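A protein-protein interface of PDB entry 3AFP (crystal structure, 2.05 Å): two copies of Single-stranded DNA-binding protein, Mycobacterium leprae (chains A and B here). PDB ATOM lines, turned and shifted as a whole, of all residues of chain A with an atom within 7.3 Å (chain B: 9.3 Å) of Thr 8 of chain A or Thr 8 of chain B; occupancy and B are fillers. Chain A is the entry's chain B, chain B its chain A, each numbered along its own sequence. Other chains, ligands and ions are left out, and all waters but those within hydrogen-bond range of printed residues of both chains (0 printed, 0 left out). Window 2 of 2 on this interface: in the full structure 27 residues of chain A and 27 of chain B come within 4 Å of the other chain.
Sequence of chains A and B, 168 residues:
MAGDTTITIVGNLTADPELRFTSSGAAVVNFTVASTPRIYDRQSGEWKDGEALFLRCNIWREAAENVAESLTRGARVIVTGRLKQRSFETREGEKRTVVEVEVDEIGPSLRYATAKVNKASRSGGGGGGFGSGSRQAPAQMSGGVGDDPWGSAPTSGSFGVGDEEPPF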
ATOM      1  N   THR A   6     -31.588 -33.501 -14.873  1.00  0.00           N
ATOM      2  CA  THR A   6     -30.294 -32.809 -14.945  1.00  0.00           C
ATOM      3  C   THR A   6     -30.437 -31.443 -15.622  1.00  0.00           C
ATOM      4  O   THR A   6     -31.458 -31.144 -16.281  1.00  0.00           O
ATOM      5  CB  THR A   6     -29.279 -33.639 -15.714  1.00  0.00           C
ATOM      6  OG1 THR A   6     -29.826 -33.996 -16.992  1.00  0.00           O
ATOM      7  CG2 THR A   6     -28.976 -34.962 -14.958  1.00  0.00           C
ATOM      8  N   ILE A   7     -29.414 -30.607 -15.463  1.00  0.00           N
ATOM      9  CA  ILE A   7     -29.479 -29.289 -15.993  1.00  0.00           C
ATOM     10  C   ILE A   7     -28.066 -28.829 -16.204  1.00  0.00           C
ATOM     11  O   ILE A   7     -27.157 -29.222 -15.453  1.00  0.00           O
ATOM     12  CB  ILE A   7     -30.224 -28.370 -14.968  1.00  0.00           C
ATOM     13  CG1 ILE A   7     -30.176 -26.909 -15.351  1.00  0.00           C
ATOM     14  CG2 ILE A   7     -29.620 -28.496 -13.539  1.00  0.00           C
ATOM     15  CD1 ILE A   7     -30.918 -25.979 -14.381  1.00  0.00           C
ATOM     16  N   THR A   8     -27.889 -27.963 -17.197  1.00  0.00           N
ATOM     17  CA  THR A   8     -26.675 -27.171 -17.352  1.00  0.00           C
ATOM     18  C   THR A   8     -27.063 -25.694 -17.229  1.00  0.00           C
ATOM     19  O   THR A   8     -27.967 -25.218 -17.927  1.00  0.00           O
ATOM     20  CB  THR A   8     -26.061 -27.394 -18.743  1.00  0.00           C
ATOM     21  OG1 THR A   8     -25.666 -28.755 -18.862  1.00  0.00           O
ATOM     22  CG2 THR A   8     -24.829 -26.481 -18.955  1.00  0.00           C
ATOM     23  N   ILE A   9     -26.394 -24.942 -16.372  1.00  0.00           N
ATOM     24  CA  ILE A   9     -26.736 -23.533 -16.239  1.00  0.00           C
ATOM     25  C   ILE A   9     -25.467 -22.723 -16.350  1.00  0.00           C
ATOM     26  O   ILE A   9     -24.408 -23.086 -15.768  1.00  0.00           O
ATOM     27  CB  ILE A   9     -27.553 -23.205 -14.946  1.00  0.00           C
ATOM     28  CG1 ILE A   9     -27.934 -21.679 -14.921  1.00  0.00           C
ATOM     29  CG2 ILE A   9     -26.823 -23.585 -13.648  1.00  0.00           C
ATOM     30  CD1 ILE A   9     -28.935 -21.317 -13.826  1.00  0.00           C
ATOM     31  N   VAL A  10     -25.537 -21.678 -17.171  1.00  0.00           N
ATOM     32  CA  VAL A  10     -24.443 -20.704 -17.318  1.00  0.00           C
ATOM     33  C   VAL A  10     -24.852 -19.366 -16.701  1.00  0.00           C
ATOM     34  O   VAL A  10     -25.964 -18.878 -16.930  1.00  0.00           O
ATOM     35  CB  VAL A  10     -24.069 -20.528 -18.780  1.00  0.00           C
ATOM     36  CG1 VAL A  10     -22.929 -19.438 -18.939  1.00  0.00           C
ATOM     37  CG2 VAL A  10     -23.597 -21.902 -19.294  1.00  0.00           C
ATOM     38  N   SER A  35     -28.442 -16.293 -14.035  1.00  0.00           N
ATOM     39  CA  SER A  35     -28.337 -16.491 -15.493  1.00  0.00           C
ATOM     40  C   SER A  35     -29.243 -15.482 -16.229  1.00  0.00           C
ATOM     41  O   SER A  35     -30.480 -15.497 -16.050  1.00  0.00           O
ATOM     42  CB  SER A  35     -28.758 -17.910 -15.869  1.00  0.00           C
ATOM     43  OG  SER A  35     -28.668 -18.076 -17.263  1.00  0.00           O
ATOM     44  N   LEU A  55     -30.679 -19.539  -9.481  1.00  0.00           N
ATOM     45  CA  LEU A  55     -30.780 -20.872  -8.939  1.00  0.00           C
ATOM     46  C   LEU A  55     -29.707 -21.047  -7.876  1.00  0.00           C
ATOM     47  O   LEU A  55     -28.520 -20.814  -8.139  1.00  0.00           O
ATOM     48  CB  LEU A  55     -30.605 -21.939 -10.029  1.00  0.00           C
ATOM     49  CG  LEU A  55     -31.706 -22.158 -11.087  1.00  0.00           C
ATOM     50  CD1 LEU A  55     -31.301 -23.260 -12.045  1.00  0.00           C
ATOM     51  CD2 LEU A  55     -33.107 -22.446 -10.502  1.00  0.00           C
ATOM     52  N   ILE A  78     -20.042 -22.383 -15.476  1.00  0.00           N
ATOM     53  CA  ILE A  78     -20.811 -23.372 -16.165  1.00  0.00           C
ATOM     54  C   ILE A  78     -21.044 -24.454 -15.116  1.00  0.00           C
ATOM     55  O   ILE A  78     -20.098 -24.946 -14.506  1.00  0.00           O
ATOM     56  CB  ILE A  78     -20.012 -24.036 -17.273  1.00  0.00           C
ATOM     57  CG1 ILE A  78     -19.391 -22.994 -18.182  1.00  0.00           C
ATOM     58  CG2 ILE A  78     -20.910 -25.051 -18.018  1.00  0.00           C
ATOM     59  CD1 ILE A  78     -18.576 -23.673 -19.339  1.00  0.00           C
ATOM     60  N   VAL A  79     -22.298 -24.814 -14.921  1.00  0.00           N
ATOM     61  CA  VAL A  79     -22.653 -25.726 -13.866  1.00  0.00           C
ATOM     62  C   VAL A  79     -23.497 -26.793 -14.439  1.00  0.00           C
ATOM     63  O   VAL A  79     -24.490 -26.494 -15.128  1.00  0.00           O
ATOM     64  CB  VAL A  79     -23.464 -25.024 -12.754  1.00  0.00           C
ATOM     65  CG1 VAL A  79     -23.921 -26.006 -11.707  1.00  0.00           C
ATOM     66  CG2 VAL A  79     -22.675 -23.787 -12.154  1.00  0.00           C
ATOM     67  N   THR A  80     -23.143 -28.046 -14.164  1.00  0.00           N
ATOM     68  CA  THR A  80     -24.073 -29.126 -14.449  1.00  0.00           C
ATOM     69  C   THR A  80     -24.477 -29.757 -13.138  1.00  0.00           C
ATOM     70  O   THR A  80     -23.648 -29.842 -12.201  1.00  0.00           O
ATOM     71  CB  THR A  80     -23.437 -30.205 -15.378  1.00  0.00           C
ATOM     72  OG1 THR A  80     -22.356 -30.854 -14.681  1.00  0.00           O
ATOM     73  CG2 THR A  80     -22.829 -29.558 -16.646  1.00  0.00           C
ATOM     74  N   GLY A  81     -25.713 -30.210 -13.051  1.00  0.00           N
ATOM     75  CA  GLY A  81     -26.139 -30.958 -11.890  1.00  0.00           C
ATOM     76  C   GLY A  81     -27.541 -31.466 -11.969  1.00  0.00           C
ATOM     77  O   GLY A  81     -28.103 -31.565 -13.054  1.00  0.00           O
ATOM     78  N   VAL A 101     -30.089 -26.752  -7.193  1.00  0.00           N
ATOM     79  CA  VAL A 101     -29.234 -27.637  -7.972  1.00  0.00           C
ATOM     80  C   VAL A 101     -28.203 -28.381  -7.091  1.00  0.00           C
ATOM     81  O   VAL A 101     -27.423 -27.745  -6.379  1.00  0.00           O
ATOM     82  CB  VAL A 101     -28.483 -26.829  -9.070  1.00  0.00           C
ATOM     83  CG1 VAL A 101     -27.642 -27.745  -9.952  1.00  0.00           C
ATOM     84  CG2 VAL A 101     -29.481 -26.009  -9.915  1.00  0.00           C
ATOM     85  N   THR B   5     -29.943 -28.737 -31.737  1.00  0.00           N
ATOM     86  CA  THR B   5     -29.854 -29.811 -30.778  1.00  0.00           C
ATOM     87  C   THR B   5     -28.642 -29.457 -29.926  1.00  0.00           C
ATOM     88  O   THR B   5     -27.520 -29.369 -30.452  1.00  0.00           O
ATOM     89  CB  THR B   5     -29.667 -31.143 -31.531  1.00  0.00           C
ATOM     90  OG1 THR B   5     -30.839 -31.386 -32.343  1.00  0.00           O
ATOM     91  CG2 THR B   5     -29.416 -32.342 -30.524  1.00  0.00           C
ATOM     92  N   THR B   6     -28.850 -29.220 -28.628  1.00  0.00           N
ATOM     93  CA  THR B   6     -27.703 -28.812 -27.778  1.00  0.00           C
ATOM     94  C   THR B   6     -27.198 -29.981 -26.956  1.00  0.00           C
ATOM     95  O   THR B   6     -27.869 -31.013 -26.849  1.00  0.00           O
ATOM     96  CB  THR B   6     -28.008 -27.597 -26.864  1.00  0.00           C
ATOM     97  OG1 THR B   6     -29.100 -27.919 -26.017  1.00  0.00           O
ATOM     98  CG2 THR B   6     -28.430 -26.402 -27.714  1.00  0.00           C
ATOM     99  N   ILE B   7     -25.966 -29.846 -26.450  1.00  0.00           N
ATOM    100  CA  ILE B   7     -25.368 -30.904 -25.700  1.00  0.00           C
ATOM    101  C   ILE B   7     -24.422 -30.340 -24.702  1.00  0.00           C
ATOM    102  O   ILE B   7     -23.801 -29.251 -24.924  1.00  0.00           O
ATOM    103  CB  ILE B   7     -24.651 -31.913 -26.645  1.00  0.00           C
ATOM    104  CG1 ILE B   7     -24.110 -33.106 -25.870  1.00  0.00           C
ATOM    105  CG2 ILE B   7     -23.492 -31.271 -27.438  1.00  0.00           C
ATOM    106  CD1 ILE B   7     -23.535 -34.154 -26.778  1.00  0.00           C
ATOM    107  N   THR B   8     -24.270 -31.072 -23.614  1.00  0.00           N
ATOM    108  CA  THR B   8     -23.227 -30.749 -22.622  1.00  0.00           C
ATOM    109  C   THR B   8     -22.347 -31.996 -22.542  1.00  0.00           C
ATOM    110  O   THR B   8     -22.864 -33.102 -22.434  1.00  0.00           O
ATOM    111  CB  THR B   8     -23.844 -30.489 -21.237  1.00  0.00           C
ATOM    112  OG1 THR B   8     -24.609 -29.292 -21.282  1.00  0.00           O
ATOM    113  CG2 THR B   8     -22.736 -30.330 -20.130  1.00  0.00           C
ATOM    114  N   ILE B   9     -21.043 -31.840 -22.614  1.00  0.00           N
ATOM    115  CA  ILE B   9     -20.155 -32.951 -22.438  1.00  0.00           C
ATOM    116  C   ILE B   9     -19.086 -32.575 -21.410  1.00  0.00           C
ATOM    117  O   ILE B   9     -18.623 -31.422 -21.401  1.00  0.00           O
ATOM    118  CB  ILE B   9     -19.506 -33.443 -23.792  1.00  0.00           C
ATOM    119  CG1 ILE B   9     -18.641 -34.693 -23.518  1.00  0.00           C
ATOM    120  CG2 ILE B   9     -18.658 -32.352 -24.492  1.00  0.00           C
ATOM    121  CD1 ILE B   9     -18.092 -35.392 -24.861  1.00  0.00           C
ATOM    122  N   VAL B  10     -18.718 -33.565 -20.567  1.00  0.00           N
ATOM    123  CA  VAL B  10     -17.657 -33.438 -19.560  1.00  0.00           C
ATOM    124  C   VAL B  10     -16.582 -34.447 -19.910  1.00  0.00           C
ATOM    125  O   VAL B  10     -16.860 -35.626 -20.094  1.00  0.00           O
ATOM    126  CB  VAL B  10     -18.232 -33.694 -18.104  1.00  0.00           C
ATOM    127  CG1 VAL B  10     -17.132 -33.620 -17.042  1.00  0.00           C
ATOM    128  CG2 VAL B  10     -19.290 -32.619 -17.798  1.00  0.00           C
ATOM    129  N   GLY B  11     -15.356 -33.992 -20.092  1.00  0.00           N
ATOM    130  CA  GLY B  11     -14.309 -34.967 -20.342  1.00  0.00           C
ATOM    131  C   GLY B  11     -12.967 -34.313 -20.340  1.00  0.00           C
ATOM    132  O   GLY B  11     -12.834 -33.218 -19.830  1.00  0.00           O
ATOM    133  N   VAL B  33     -12.793 -33.489 -27.037  1.00  0.00           N
ATOM    134  CA  VAL B  33     -13.077 -33.881 -25.636  1.00  0.00           C
ATOM    135  C   VAL B  33     -13.287 -35.389 -25.603  1.00  0.00           C
ATOM    136  O   VAL B  33     -14.139 -35.931 -26.350  1.00  0.00           O
ATOM    137  CB  VAL B  33     -14.326 -33.130 -25.087  1.00  0.00           C
ATOM    138  CG1 VAL B  33     -14.694 -33.566 -23.699  1.00  0.00           C
ATOM    139  CG2 VAL B  33     -14.055 -31.584 -25.115  1.00  0.00           C
ATOM    140  N   SER B  35     -14.651 -38.169 -23.324  1.00  0.00           N
ATOM    141  CA  SER B  35     -15.429 -38.450 -22.146  1.00  0.00           C
ATOM    142  C   SER B  35     -15.502 -39.964 -21.935  1.00  0.00           C
ATOM    143  O   SER B  35     -16.027 -40.701 -22.788  1.00  0.00           O
ATOM    144  CB  SER B  35     -16.834 -37.928 -22.337  1.00  0.00           C
ATOM    145  OG  SER B  35     -17.620 -38.384 -21.279  1.00  0.00           O
ATOM    146  N   LEU B  53     -16.423 -41.456 -25.391  1.00  0.00           N
ATOM    147  CA  LEU B  53     -17.013 -40.638 -26.453  1.00  0.00           C
ATOM    148  C   LEU B  53     -16.013 -39.500 -26.734  1.00  0.00           C
ATOM    149  O   LEU B  53     -15.603 -38.791 -25.794  1.00  0.00           O
ATOM    150  CB  LEU B  53     -18.364 -40.116 -25.973  1.00  0.00           C
ATOM    151  CG  LEU B  53     -19.122 -39.088 -26.824  1.00  0.00           C
ATOM    152  CD1 LEU B  53     -19.590 -39.716 -28.155  1.00  0.00           C
ATOM    153  CD2 LEU B  53     -20.373 -38.541 -26.080  1.00  0.00           C
ATOM    154  N   LEU B  55     -15.645 -36.132 -28.762  1.00  0.00           N
ATOM    155  CA  LEU B  55     -16.319 -35.121 -29.559  1.00  0.00           C
ATOM    156  C   LEU B  55     -15.367 -34.027 -30.002  1.00  0.00           C
ATOM    157  O   LEU B  55     -14.736 -33.375 -29.193  1.00  0.00           O
ATOM    158  CB  LEU B  55     -17.546 -34.527 -28.892  1.00  0.00           C
ATOM    159  CG  LEU B  55     -18.747 -35.438 -28.599  1.00  0.00           C
ATOM    160  CD1 LEU B  55     -19.879 -34.662 -27.977  1.00  0.00           C
ATOM    161  CD2 LEU B  55     -19.273 -36.181 -29.880  1.00  0.00           C
ATOM    162  N   CYS B  57     -14.598 -30.452 -31.177  1.00  0.00           N
ATOM    163  CA  CYS B  57     -15.144 -29.164 -30.808  1.00  0.00           C
ATOM    164  C   CYS B  57     -14.430 -28.000 -31.506  1.00  0.00           C
ATOM    165  O   CYS B  57     -13.226 -28.075 -31.786  1.00  0.00           O
ATOM    166  CB  CYS B  57     -15.019 -28.975 -29.278  1.00  0.00           C
ATOM    167  SG  CYS B  57     -15.922 -30.230 -28.270  1.00  0.00           S
ATOM    168  N   VAL B  77     -12.776 -30.749 -18.645  1.00  0.00           N
ATOM    169  CA  VAL B  77     -13.533 -29.590 -19.074  1.00  0.00           C
ATOM    170  C   VAL B  77     -15.004 -29.887 -19.099  1.00  0.00           C
ATOM    171  O   VAL B  77     -15.430 -31.036 -19.235  1.00  0.00           O
ATOM    172  CB  VAL B  77     -13.072 -29.061 -20.472  1.00  0.00           C
ATOM    173  CG1 VAL B  77     -11.581 -28.590 -20.409  1.00  0.00           C
ATOM    174  CG2 VAL B  77     -13.223 -30.169 -21.561  1.00  0.00           C
ATOM    175  N   ILE B  78     -15.786 -28.831 -18.962  1.00  0.00           N
ATOM    176  CA  ILE B  78     -17.228 -28.920 -19.086  1.00  0.00           C
ATOM    177  C   ILE B  78     -17.515 -28.104 -20.359  1.00  0.00           C
ATOM    178  O   ILE B  78     -17.091 -26.967 -20.447  1.00  0.00           O
ATOM    179  CB  ILE B  78     -17.947 -28.248 -17.933  1.00  0.00           C
ATOM    180  CG1 ILE B  78     -17.507 -28.867 -16.607  1.00  0.00           C
ATOM    181  CG2 ILE B  78     -19.478 -28.474 -18.091  1.00  0.00           C
ATOM    182  CD1 ILE B  78     -17.728 -27.902 -15.467  1.00  0.00           C
ATOM    183  N   VAL B  79     -18.172 -28.725 -21.333  1.00  0.00           N
ATOM    184  CA  VAL B  79     -18.401 -28.060 -22.613  1.00  0.00           C
ATOM    185  C   VAL B  79     -19.864 -28.120 -22.961  1.00  0.00           C
ATOM    186  O   VAL B  79     -20.484 -29.163 -22.865  1.00  0.00           O
ATOM    187  CB  VAL B  79     -17.610 -28.708 -23.736  1.00  0.00           C
ATOM    188  CG1 VAL B  79     -18.041 -28.158 -25.086  1.00  0.00           C
ATOM    189  CG2 VAL B  79     -16.089 -28.486 -23.530  1.00  0.00           C
ATOM    190  N   THR B  80     -20.416 -26.987 -23.362  1.00  0.00           N
ATOM    191  CA  THR B  80     -21.818 -26.978 -23.832  1.00  0.00           C
ATOM    192  C   THR B  80     -21.854 -26.320 -25.221  1.00  0.00           C
ATOM    193  O   THR B  80     -21.064 -25.391 -25.492  1.00  0.00           O
ATOM    194  CB  THR B  80     -22.699 -26.195 -22.853  1.00  0.00           C
ATOM    195  OG1 THR B  80     -24.074 -26.438 -23.166  1.00  0.00           O
ATOM    196  CG2 THR B  80     -22.439 -24.702 -23.004  1.00  0.00           C
ATOM    197  N   GLY B  81     -22.717 -26.810 -26.109  1.00  0.00           N
ATOM    198  CA  GLY B  81     -22.873 -26.172 -27.397  1.00  0.00           C
ATOM    199  C   GLY B  81     -23.804 -26.911 -28.314  1.00  0.00           C
ATOM    200  O   GLY B  81     -24.628 -27.690 -27.852  1.00  0.00           O
ATOM    201  N   ARG B  82     -23.700 -26.643 -29.605  1.00  0.00           N
ATOM    202  CA  ARG B  82     -24.678 -27.183 -30.561  1.00  0.00           C
ATOM    203  C   ARG B  82     -24.036 -28.316 -31.324  1.00  0.00           C
ATOM    204  O   ARG B  82     -22.878 -28.212 -31.736  1.00  0.00           O
ATOM    205  CB  ARG B  82     -25.127 -26.087 -31.535  1.00  0.00           C
ATOM    206  CG  ARG B  82     -26.079 -25.064 -30.871  1.00  0.00           C
ATOM    207  CD  ARG B  82     -25.414 -23.718 -30.583  1.00  0.00           C
ATOM    208  NE  ARG B  82     -25.048 -23.040 -31.810  1.00  0.00           N
ATOM    209  CZ  ARG B  82     -23.890 -22.418 -31.992  1.00  0.00           C
ATOM    210  NH1 ARG B  82     -22.974 -22.396 -31.007  1.00  0.00           N
ATOM    211  NH2 ARG B  82     -23.654 -21.843 -33.172  1.00  0.00           N
ATOM    212  N   LEU B  83     -24.786 -29.389 -31.507  1.00  0.00           N
ATOM    213  CA  LEU B  83     -24.264 -30.560 -32.189  1.00  0.00           C
ATOM    214  C   LEU B  83     -24.505 -30.392 -33.701  1.00  0.00           C
ATOM    215  O   LEU B  83     -25.625 -30.194 -34.125  1.00  0.00           O
ATOM    216  CB  LEU B  83     -25.056 -31.794 -31.733  1.00  0.00           C
ATOM    217  CG  LEU B  83     -24.384 -33.015 -31.192  1.00  0.00           C
ATOM    218  CD1 LEU B  83     -25.314 -34.239 -31.355  1.00  0.00           C
ATOM    219  CD2 LEU B  83     -22.972 -33.304 -31.717  1.00  0.00           C
ATOM    220  N   VAL B 101     -19.000 -30.256 -32.187  1.00  0.00           N
ATOM    221  CA  VAL B 101     -19.745 -29.378 -31.309  1.00  0.00           C
ATOM    222  C   VAL B 101     -19.277 -27.964 -31.557  1.00  0.00           C
ATOM    223  O   VAL B 101     -18.096 -27.648 -31.385  1.00  0.00           O
ATOM    224  CB  VAL B 101     -19.502 -29.743 -29.809  1.00  0.00           C
ATOM    225  CG1 VAL B 101     -20.189 -28.718 -28.833  1.00  0.00           C
ATOM    226  CG2 VAL B 101     -19.966 -31.216 -29.519  1.00  0.00           C
ATOM    227  N   ASP B 104     -20.602 -23.218 -27.181  1.00  0.00           N
ATOM    228  CA  ASP B 104     -21.174 -22.025 -26.638  1.00  0.00           C
ATOM    229  C   ASP B 104     -20.385 -21.573 -25.381  1.00  0.00           C
ATOM    230  O   ASP B 104     -20.035 -20.391 -25.231  1.00  0.00           O
ATOM    231  CB  ASP B 104     -22.653 -22.262 -26.257  1.00  0.00           C
ATOM    232  CG  ASP B 104     -23.555 -22.366 -27.474  1.00  0.00           C
ATOM    233  OD1 ASP B 104     -23.277 -21.660 -28.472  1.00  0.00           O
ATOM    234  OD2 ASP B 104     -24.553 -23.143 -27.446  1.00  0.00           O
ATOM    235  N   GLU B 105     -20.108 -22.510 -24.473  1.00  0.00           N
ATOM    236  CA  GLU B 105     -19.334 -22.201 -23.270  1.00  0.00           C
ATOM    237  C   GLU B 105     -18.412 -23.371 -22.928  1.00  0.00           C
ATOM    238  O   GLU B 105     -18.747 -24.536 -23.175  1.00  0.00           O
ATOM    239  CB  GLU B 105     -20.264 -21.948 -22.063  1.00  0.00           C
ATOM    240  CG  GLU B 105     -21.283 -20.870 -22.233  1.00  0.00           C
ATOM    241  CD  GLU B 105     -20.833 -19.443 -21.887  1.00  0.00           C
ATOM    242  OE1 GLU B 105     -19.789 -19.165 -21.251  1.00  0.00           O
ATOM    243  OE2 GLU B 105     -21.616 -18.572 -22.224  1.00  0.00           O
ATOM    244  N   ILE B 106     -17.235 -23.061 -22.402  1.00  0.00           N
ATOM    245  CA  ILE B 106     -16.310 -24.090 -21.949  1.00  0.00           C
ATOM    246  C   ILE B 106     -15.554 -23.543 -20.705  1.00  0.00           C
ATOM    247  O   ILE B 106     -15.249 -22.363 -20.631  1.00  0.00           O
ATOM    248  CB  ILE B 106     -15.279 -24.502 -23.007  1.00  0.00           C
ATOM    249  CG1 ILE B 106     -14.206 -25.380 -22.382  1.00  0.00           C
ATOM    250  CG2 ILE B 106     -14.522 -23.219 -23.618  1.00  0.00           C
ATOM    251  CD1 ILE B 106     -13.415 -26.185 -23.409  1.00  0.00           C
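No residue of chain B comes within 4 Å of Ile 7 of chain A.
Thr 8 of chain A touches just one residue of chain B: Thr 8.
Of the printed residues of chain B, Val 10 of chain A touches Glu 105.
Of the printed residues of chain B, Ile 78 of chain A touches Ile 78 (3.7 Å), Glu 105 (3.6 Å) and Ile 106 (3.3 Å).
Of the printed residues of chain B, Thr 80 of chain A touches Thr 8 and Ile 78.
Thr 6 of chain B touches none of the printed residues of chain A.
Of the printed residues of chain A, Thr 8 of chain B touches Thr 8 and Thr 80.
Of the printed residues of chain A, Ile 78 of chain B touches Ile 78 and Thr 80.
Printed residues of chain A within 4 Å of Ile 106 of chain B: Ile 78.
The nearest residue of chain B that does not touch Thr 8 of chain A is Thr 80 of chain B (4.3 Å).
The nearest residue of chain A that does not touch Thr 8 of chain B is Ile 78 of chain A (6.0 Å).
The nearest printed residue of chain B that does not touch Val 10 of chain A is Thr 80 of chain B (4.8 Å).
Thr 8 of chain A touches its own counterpart, Thr 8 of chain B.
Ile 78 of chain A touches its own counterpart, Ile 78 of chain B.
Thr 80 of chain A touches Thr 8 of chain B, but with the chains exchanged Thr 8 of chain A does not touch Thr 80 of chain B (4.3 Å).
Thr 80 of chain A touches Ile 78 of chain B, but with the chains exchanged Ile 78 of chain A does not touch Thr 80 of chain B (5.2 Å).
Positions printed for both chains: 6, 7, 8, 9, 10, 35, 55, 78, 79, 80, 81 and 101.
Among the printed residues, pairs that only touch across the chains: Val 10 of chain A with Glu 105 of chain B (3.6 Å), Ile 78 of chain A with Ile 78 of chain B (3.7 Å), Ile 78 of chain A with Glu 105 of chain B (3.6 Å), Ile 78 of chain A with Ile 106 of chain B (3.3 Å), Thr 80 of chain A with Thr 8 of chain B (3.6 Å) and Thr 80 of chain A with Ile 78 of chain B (3.8 Å).
N of Thr 80 of chain B is in hydrogen-bond range of O of Glu 105 of chain B, 3.0 Å away.
OG1 of Thr 80 of chain B lies within hydrogen-bond range of OG1 of Thr 8 of chain B, at 3.5 Å.
The backbone carbonyl oxygen (O) of Val 10 of chain A sits at hydrogen-bond distance from the side-chain hydroxyl (OG) of Ser 35 of chain A (2.8 Å).
OG1 of Thr 8 of chain B sits at hydrogen-bond distance from OG1 of Thr 8 of chain A, 2.7 Å away.
Of the 12 printed residues of chain A, 4 touch a printed residue of chain B.
Among the printed residues, 7 pairs touch across the chains.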
